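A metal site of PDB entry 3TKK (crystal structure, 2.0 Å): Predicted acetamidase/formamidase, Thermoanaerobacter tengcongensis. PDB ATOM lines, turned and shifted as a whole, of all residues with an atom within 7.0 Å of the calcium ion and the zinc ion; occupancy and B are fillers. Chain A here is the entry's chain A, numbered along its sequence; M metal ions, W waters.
Of the 24 residues printed, 4 come within 4 Å of the calcium ion.
Merely in contact with the zinc ion: Glu 193 (3.97 Å).
Five residues have an atom within 4 Å of the zinc ion: CSD 39, Asp 184, His 186, Glu 193 and Glu 200.
The calcium ion is bound by the side-chain amide oxygen (OD1) of Asn 157 (2.3 Å), the side-chain carboxylate (OD2) of Asp 184 (2.3 Å), the side-chain carboxylate (OD1) of Asp 159 (2.3 Å), water W3 (2.5 Å), water W2 (2.5 Å), water W1 (2.5 Å) and the side-chain carboxylate (OD2) of Asp 159 (2.6 Å).
The zinc ion is bound by water W1 (2.0 Å), NE2 of His 186 (2.1 Å), OE1 of Glu 200 (2.1 Å), OD1 of Asp 184 (2.1 Å), OD2 of CSD 39 (2.2 Å) and OE2 of Glu 200 (2.2 Å).
A ring nitrogen (ND1) of His 186 sits at hydrogen-bond distance from the side-chain sulfur (SD) of Met 189 (3.5 Å).
The backbone NH (N) of Gly 198 lies close to the side-chain carboxylate (OE2) of Glu 200.
O of Asp 184 is in hydrogen-bond range of N of Gly 135 (3.0 Å).
The backbone NH (N) of Asn 60 is in hydrogen-bond range of O of CSD 39 (2.7 Å).
The backbone carbonyl oxygen (O) of Gly 149 is in hydrogen-bond range of the side-chain amide nitrogen (ND2) of Asn 157 (3.0 Å).
The side-chain carboxylate (OD2) of Asp 159 lies close to the side-chain carboxylate (OE1) of Glu 193.
N of Asp 159 lies within hydrogen-bond range of O of Gly 135.
OE2 of Glu 193 is in hydrogen-bond range of N of Gly 198 (3.3 Å).
Water W2 bridges OD1 of CSD 39 (3.2 Å) and OD1 of Asn 60 (3.4 Å).
Water W3 lies within hydrogen-bond range of OD1 of Asp 280 and ND2 of Asn 157.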
ATOM      1  N   ASP A  38      -3.884  12.182  23.367  1.00  0.00           N
ATOM      2  CA  ASP A  38      -4.342  10.898  23.926  1.00  0.00           C
ATOM      3  C   ASP A  38      -5.222  10.208  22.944  1.00  0.00           C
ATOM      4  O   ASP A  38      -5.593  10.807  21.920  1.00  0.00           O
ATOM      5  CB  ASP A  38      -5.037  11.040  25.300  1.00  0.00           C
ATOM      6  CG  ASP A  38      -6.246  11.988  25.274  1.00  0.00           C
ATOM      7  OD1 ASP A  38      -7.134  11.802  24.396  1.00  0.00           O
ATOM      8  OD2 ASP A  38      -6.339  12.905  26.156  1.00  0.00           O
ATOM      9  N   CSD A  39      -5.635   8.974  23.324  1.00  0.00           N
ATOM     10  CA  CSD A  39      -6.615   8.007  22.702  1.00  0.00           C
ATOM     11  CB  CSD A  39      -6.801   6.847  23.794  1.00  0.00           C
ATOM     12  SG  CSD A  39      -7.821   5.181  24.030  1.00  0.00           S
ATOM     13  C   CSD A  39      -7.908   8.798  22.385  1.00  0.00           C
ATOM     14  O   CSD A  39      -8.661   8.478  21.416  1.00  0.00           O
ATOM     15  OD1 CSD A  39      -8.949   4.857  23.104  1.00  0.00           O
ATOM     16  OD2 CSD A  39      -7.035   3.913  24.176  1.00  0.00           O
ATOM     17  N   PHE A  40      -8.235   9.807  23.208  1.00  0.00           N
ATOM     18  CA  PHE A  40      -9.446  10.609  22.933  1.00  0.00           C
ATOM     19  C   PHE A  40      -9.279  11.980  22.191  1.00  0.00           C
ATOM     20  O   PHE A  40     -10.126  12.852  22.332  1.00  0.00           O
ATOM     21  CB  PHE A  40     -10.268  10.766  24.228  1.00  0.00           C
ATOM     22  CG  PHE A  40     -10.515   9.454  24.982  1.00  0.00           C
ATOM     23  CD1 PHE A  40      -9.945   9.237  26.268  1.00  0.00           C
ATOM     24  CD2 PHE A  40     -11.320   8.465  24.431  1.00  0.00           C
ATOM     25  CE1 PHE A  40     -10.229   8.050  26.993  1.00  0.00           C
ATOM     26  CE2 PHE A  40     -11.593   7.234  25.143  1.00  0.00           C
ATOM     27  CZ  PHE A  40     -11.044   7.032  26.414  1.00  0.00           C
ATOM     28  N   ASN A  60      -8.095   7.450  18.952  1.00  0.00           N
ATOM     29  CA  ASN A  60      -6.744   6.938  18.592  1.00  0.00           C
ATOM     30  C   ASN A  60      -5.966   7.684  17.504  1.00  0.00           C
ATOM     31  O   ASN A  60      -5.406   6.983  16.603  1.00  0.00           O
ATOM     32  CB  ASN A  60      -6.791   5.483  18.086  1.00  0.00           C
ATOM     33  CG  ASN A  60      -7.273   4.529  19.128  1.00  0.00           C
ATOM     34  OD1 ASN A  60      -8.282   3.793  18.943  1.00  0.00           O
ATOM     35  ND2 ASN A  60      -6.586   4.539  20.238  1.00  0.00           N
ATOM     36  N   GLY A 135       0.665   2.634  23.189  1.00  0.00           N
ATOM     37  CA  GLY A 135      -0.363   1.652  22.859  1.00  0.00           C
ATOM     38  C   GLY A 135      -0.541   1.391  21.349  1.00  0.00           C
ATOM     39  O   GLY A 135      -0.843   0.272  20.944  1.00  0.00           O
ATOM     40  N   VAL A 136      -0.442   2.454  20.527  1.00  0.00           N
ATOM     41  CA  VAL A 136      -0.713   2.377  19.077  1.00  0.00           C
ATOM     42  C   VAL A 136       0.660   2.715  18.415  1.00  0.00           C
ATOM     43  O   VAL A 136       1.246   3.802  18.620  1.00  0.00           O
ATOM     44  CB  VAL A 136      -1.721   3.384  18.710  1.00  0.00           C
ATOM     45  CG1 VAL A 136      -1.739   3.670  17.178  1.00  0.00           C
ATOM     46  CG2 VAL A 136      -3.190   2.869  19.087  1.00  0.00           C
ATOM     47  N   CYS A 148      -6.951   2.838  13.298  1.00  0.00           N
ATOM     48  CA  CYS A 148      -6.065   2.996  14.450  1.00  0.00           C
ATOM     49  C   CYS A 148      -6.314   2.160  15.676  1.00  0.00           C
ATOM     50  O   CYS A 148      -5.367   1.820  16.364  1.00  0.00           O
ATOM     51  CB  CYS A 148      -6.032   4.491  14.850  1.00  0.00           C
ATOM     52  SG  CYS A 148      -4.945   5.205  13.676  1.00  0.00           S
ATOM     53  N   GLY A 149      -7.580   1.867  15.950  1.00  0.00           N
ATOM     54  CA  GLY A 149      -7.989   1.029  17.104  1.00  0.00           C
ATOM     55  C   GLY A 149      -7.835  -0.483  16.877  1.00  0.00           C
ATOM     56  O   GLY A 149      -8.154  -1.270  17.765  1.00  0.00           O
ATOM     57  N   ASN A 157      -2.984  -0.931  17.176  1.00  0.00           N
ATOM     58  CA  ASN A 157      -3.398  -0.796  18.615  1.00  0.00           C
ATOM     59  C   ASN A 157      -3.127  -2.137  19.303  1.00  0.00           C
ATOM     60  O   ASN A 157      -4.037  -2.910  19.646  1.00  0.00           O
ATOM     61  CB  ASN A 157      -4.897  -0.539  18.656  1.00  0.00           C
ATOM     62  CG  ASN A 157      -5.392  -0.155  20.051  1.00  0.00           C
ATOM     63  OD1 ASN A 157      -4.654   0.239  20.931  1.00  0.00           O
ATOM     64  ND2 ASN A 157      -6.707  -0.281  20.249  1.00  0.00           N
ATOM     65  N   MET A 158      -1.878  -2.362  19.538  1.00  0.00           N
ATOM     66  CA  MET A 158      -1.417  -3.594  20.149  1.00  0.00           C
ATOM     67  C   MET A 158      -1.402  -3.559  21.702  1.00  0.00           C
ATOM     68  O   MET A 158      -1.219  -4.613  22.276  1.00  0.00           O
ATOM     69  CB  MET A 158      -0.002  -3.888  19.670  1.00  0.00           C
ATOM     70  CG  MET A 158       0.205  -3.996  18.204  1.00  0.00           C
ATOM     71  SD  MET A 158       1.903  -4.470  17.740  1.00  0.00           S
ATOM     72  CE  MET A 158       2.603  -2.830  17.835  1.00  0.00           C
ATOM     73  N   ASP A 159      -1.443  -2.349  22.338  1.00  0.00           N
ATOM     74  CA  ASP A 159      -1.530  -2.149  23.808  1.00  0.00           C
ATOM     75  C   ASP A 159      -0.658  -3.165  24.489  1.00  0.00           C
ATOM     76  O   ASP A 159      -1.073  -3.944  25.401  1.00  0.00           O
ATOM     77  CB  ASP A 159      -2.945  -2.200  24.379  1.00  0.00           C
ATOM     78  CG  ASP A 159      -3.801  -0.940  23.991  1.00  0.00           C
ATOM     79  OD1 ASP A 159      -3.301   0.158  23.645  1.00  0.00           O
ATOM     80  OD2 ASP A 159      -5.011  -1.135  23.787  1.00  0.00           O
ATOM     81  N   ASP A 184      -1.583   7.033  21.340  1.00  0.00           N
ATOM     82  CA  ASP A 184      -2.219   6.335  22.476  1.00  0.00           C
ATOM     83  C   ASP A 184      -1.304   5.982  23.535  1.00  0.00           C
ATOM     84  O   ASP A 184      -1.293   4.766  23.897  1.00  0.00           O
ATOM     85  CB  ASP A 184      -2.879   5.028  21.883  1.00  0.00           C
ATOM     86  CG  ASP A 184      -3.604   4.181  22.908  1.00  0.00           C
ATOM     87  OD1 ASP A 184      -4.285   4.730  23.746  1.00  0.00           O
ATOM     88  OD2 ASP A 184      -3.583   2.908  22.901  1.00  0.00           O
ATOM     89  N   LEU A 185      -0.526   6.960  24.066  1.00  0.00           N
ATOM     90  CA  LEU A 185       0.312   6.710  25.169  1.00  0.00           C
ATOM     91  C   LEU A 185      -0.484   6.429  26.448  1.00  0.00           C
ATOM     92  O   LEU A 185      -1.640   6.929  26.598  1.00  0.00           O
ATOM     93  CB  LEU A 185       1.365   7.859  25.485  1.00  0.00           C
ATOM     94  CG  LEU A 185       2.190   8.511  24.345  1.00  0.00           C
ATOM     95  CD1 LEU A 185       3.207   9.735  24.833  1.00  0.00           C
ATOM     96  CD2 LEU A 185       2.971   7.539  23.593  1.00  0.00           C
ATOM     97  N   HIS A 186       0.174   5.647  27.353  1.00  0.00           N
ATOM     98  CA  HIS A 186      -0.475   5.292  28.656  1.00  0.00           C
ATOM     99  C   HIS A 186       0.563   5.586  29.678  1.00  0.00           C
ATOM    100  O   HIS A 186       1.704   5.281  29.387  1.00  0.00           O
ATOM    101  CB  HIS A 186      -0.888   3.825  28.817  1.00  0.00           C
ATOM    102  CG  HIS A 186      -1.908   3.359  27.824  1.00  0.00           C
ATOM    103  ND1 HIS A 186      -1.965   2.068  27.390  1.00  0.00           N
ATOM    104  CD2 HIS A 186      -2.919   4.009  27.229  1.00  0.00           C
ATOM    105  CE1 HIS A 186      -2.884   1.961  26.447  1.00  0.00           C
ATOM    106  NE2 HIS A 186      -3.479   3.142  26.345  1.00  0.00           N
ATOM    107  N   MET A 189      -0.458   0.775  32.485  1.00  0.00           N
ATOM    108  CA  MET A 189      -1.516  -0.147  32.004  1.00  0.00           C
ATOM    109  C   MET A 189      -1.020  -1.551  32.420  1.00  0.00           C
ATOM    110  O   MET A 189       0.192  -1.840  32.365  1.00  0.00           O
ATOM    111  CB  MET A 189      -1.650  -0.071  30.430  1.00  0.00           C
ATOM    112  CG  MET A 189      -2.888  -0.950  29.893  1.00  0.00           C
ATOM    113  SD  MET A 189      -2.666  -1.234  28.131  1.00  0.00           S
ATOM    114  CE  MET A 189      -1.466  -2.542  28.261  1.00  0.00           C
ATOM    115  N   GLU A 193      -5.352  -5.249  29.892  1.00  0.00           N
ATOM    116  CA  GLU A 193      -6.054  -3.915  29.800  1.00  0.00           C
ATOM    117  C   GLU A 193      -7.534  -4.121  30.122  1.00  0.00           C
ATOM    118  O   GLU A 193      -8.446  -3.634  29.332  1.00  0.00           O
ATOM    119  CB  GLU A 193      -5.903  -3.254  28.385  1.00  0.00           C
ATOM    120  CG  GLU A 193      -6.378  -1.715  28.426  1.00  0.00           C
ATOM    121  CD  GLU A 193      -6.045  -1.084  27.071  1.00  0.00           C
ATOM    122  OE1 GLU A 193      -6.039  -1.900  26.080  1.00  0.00           O
ATOM    123  OE2 GLU A 193      -5.792   0.165  27.022  1.00  0.00           O
ATOM    124  N   VAL A 196     -10.770  -1.893  29.883  1.00  0.00           N
ATOM    125  CA  VAL A 196     -10.904  -1.241  28.547  1.00  0.00           C
ATOM    126  C   VAL A 196      -9.808  -0.182  28.274  1.00  0.00           C
ATOM    127  O   VAL A 196      -9.389   0.058  27.111  1.00  0.00           O
ATOM    128  CB  VAL A 196     -12.319  -0.732  28.224  1.00  0.00           C
ATOM    129  CG1 VAL A 196     -12.587   0.783  28.447  1.00  0.00           C
ATOM    130  CG2 VAL A 196     -12.647  -0.976  26.676  1.00  0.00           C
ATOM    131  N   SER A 197      -9.269   0.462  29.291  1.00  0.00           N
ATOM    132  CA  SER A 197      -8.352   1.505  28.962  1.00  0.00           C
ATOM    133  C   SER A 197      -7.149   1.481  29.887  1.00  0.00           C
ATOM    134  O   SER A 197      -7.051   0.828  30.882  1.00  0.00           O
ATOM    135  CB  SER A 197      -8.955   2.977  29.095  1.00  0.00           C
ATOM    136  OG  SER A 197      -8.768   3.311  30.532  1.00  0.00           O
ATOM    137  N   GLY A 198      -6.177   2.254  29.489  1.00  0.00           N
ATOM    138  CA  GLY A 198      -4.971   2.533  30.275  1.00  0.00           C
ATOM    139  C   GLY A 198      -5.175   3.839  30.997  1.00  0.00           C
ATOM    140  O   GLY A 198      -6.265   4.330  31.024  1.00  0.00           O
ATOM    141  N   VAL A 199      -4.172   4.337  31.720  1.00  0.00           N
ATOM    142  CA  VAL A 199      -4.132   5.744  32.075  1.00  0.00           C
ATOM    143  C   VAL A 199      -3.761   6.552  30.757  1.00  0.00           C
ATOM    144  O   VAL A 199      -2.567   6.737  30.365  1.00  0.00           O
ATOM    145  CB  VAL A 199      -3.180   6.048  33.275  1.00  0.00           C
ATOM    146  CG1 VAL A 199      -3.226   7.630  33.620  1.00  0.00           C
ATOM    147  CG2 VAL A 199      -3.500   5.173  34.546  1.00  0.00           C
ATOM    148  N   GLU A 200      -4.812   6.999  30.082  1.00  0.00           N
ATOM    149  CA  GLU A 200      -4.735   7.565  28.736  1.00  0.00           C
ATOM    150  C   GLU A 200      -4.151   8.988  28.855  1.00  0.00           C
ATOM    151  O   GLU A 200      -4.672   9.860  29.542  1.00  0.00           O
ATOM    152  CB  GLU A 200      -6.110   7.667  28.130  1.00  0.00           C
ATOM    153  CG  GLU A 200      -6.845   6.326  28.019  1.00  0.00           C
ATOM    154  CD  GLU A 200      -6.128   5.287  27.157  1.00  0.00           C
ATOM    155  OE1 GLU A 200      -5.301   5.674  26.253  1.00  0.00           O
ATOM    156  OE2 GLU A 200      -6.426   4.009  27.213  1.00  0.00           O
ATOM    157  N   VAL A 201      -3.030   9.203  28.223  1.00  0.00           N
ATOM    158  CA  VAL A 201      -2.465  10.540  28.316  1.00  0.00           C
ATOM    159  C   VAL A 201      -1.870  11.036  26.990  1.00  0.00           C
ATOM    160  O   VAL A 201      -1.494  10.244  26.176  1.00  0.00           O
ATOM    161  CB  VAL A 201      -1.238  10.515  29.259  1.00  0.00           C
ATOM    162  CG1 VAL A 201      -1.644  10.129  30.716  1.00  0.00           C
ATOM    163  CG2 VAL A 201      -0.229   9.425  28.766  1.00  0.00           C
ATOM    164  N   GLN A 277      -3.605  -7.574  25.274  1.00  0.00           N
ATOM    165  CA  GLN A 277      -4.857  -6.977  25.588  1.00  0.00           C
ATOM    166  C   GLN A 277      -5.909  -7.880  25.118  1.00  0.00           C
ATOM    167  O   GLN A 277      -5.741  -8.586  24.071  1.00  0.00           O
ATOM    168  CB  GLN A 277      -5.085  -5.552  24.943  1.00  0.00           C
ATOM    169  CG  GLN A 277      -4.876  -5.423  23.439  1.00  0.00           C
ATOM    170  CD  GLN A 277      -6.076  -5.937  22.676  1.00  0.00           C
ATOM    171  OE1 GLN A 277      -7.211  -5.904  23.231  1.00  0.00           O
ATOM    172  NE2 GLN A 277      -5.892  -6.158  21.348  1.00  0.00           N
ATOM    173  N   ASP A 280      -9.669  -5.189  22.733  1.00  0.00           N
ATOM    174  CA  ASP A 280      -9.761  -4.404  21.497  1.00  0.00           C
ATOM    175  C   ASP A 280     -10.481  -5.292  20.455  1.00  0.00           C
ATOM    176  O   ASP A 280     -10.909  -6.452  20.745  1.00  0.00           O
ATOM    177  CB  ASP A 280      -8.369  -3.871  20.974  1.00  0.00           C
ATOM    178  CG  ASP A 280      -7.619  -2.923  22.018  1.00  0.00           C
ATOM    179  OD1 ASP A 280      -8.339  -2.169  22.693  1.00  0.00           O
ATOM    180  OD2 ASP A 280      -6.343  -2.899  22.126  1.00  0.00           O
HETATM  181 CA    CA M   1      -5.236   1.264  22.903  1.00  0.00          CA
HETATM  182 ZN    ZN M   2      -5.246   3.738  25.370  1.00  0.00          ZN
HETATM  183  O   HOH W   1      -6.180   1.937  25.117  1.00  0.00           O
HETATM  184  O   HOH W   2      -6.831   2.854  21.843  1.00  0.00           O
HETATM  185  O   HOH W   3      -7.535   0.390  22.843  1.00  0.00           O
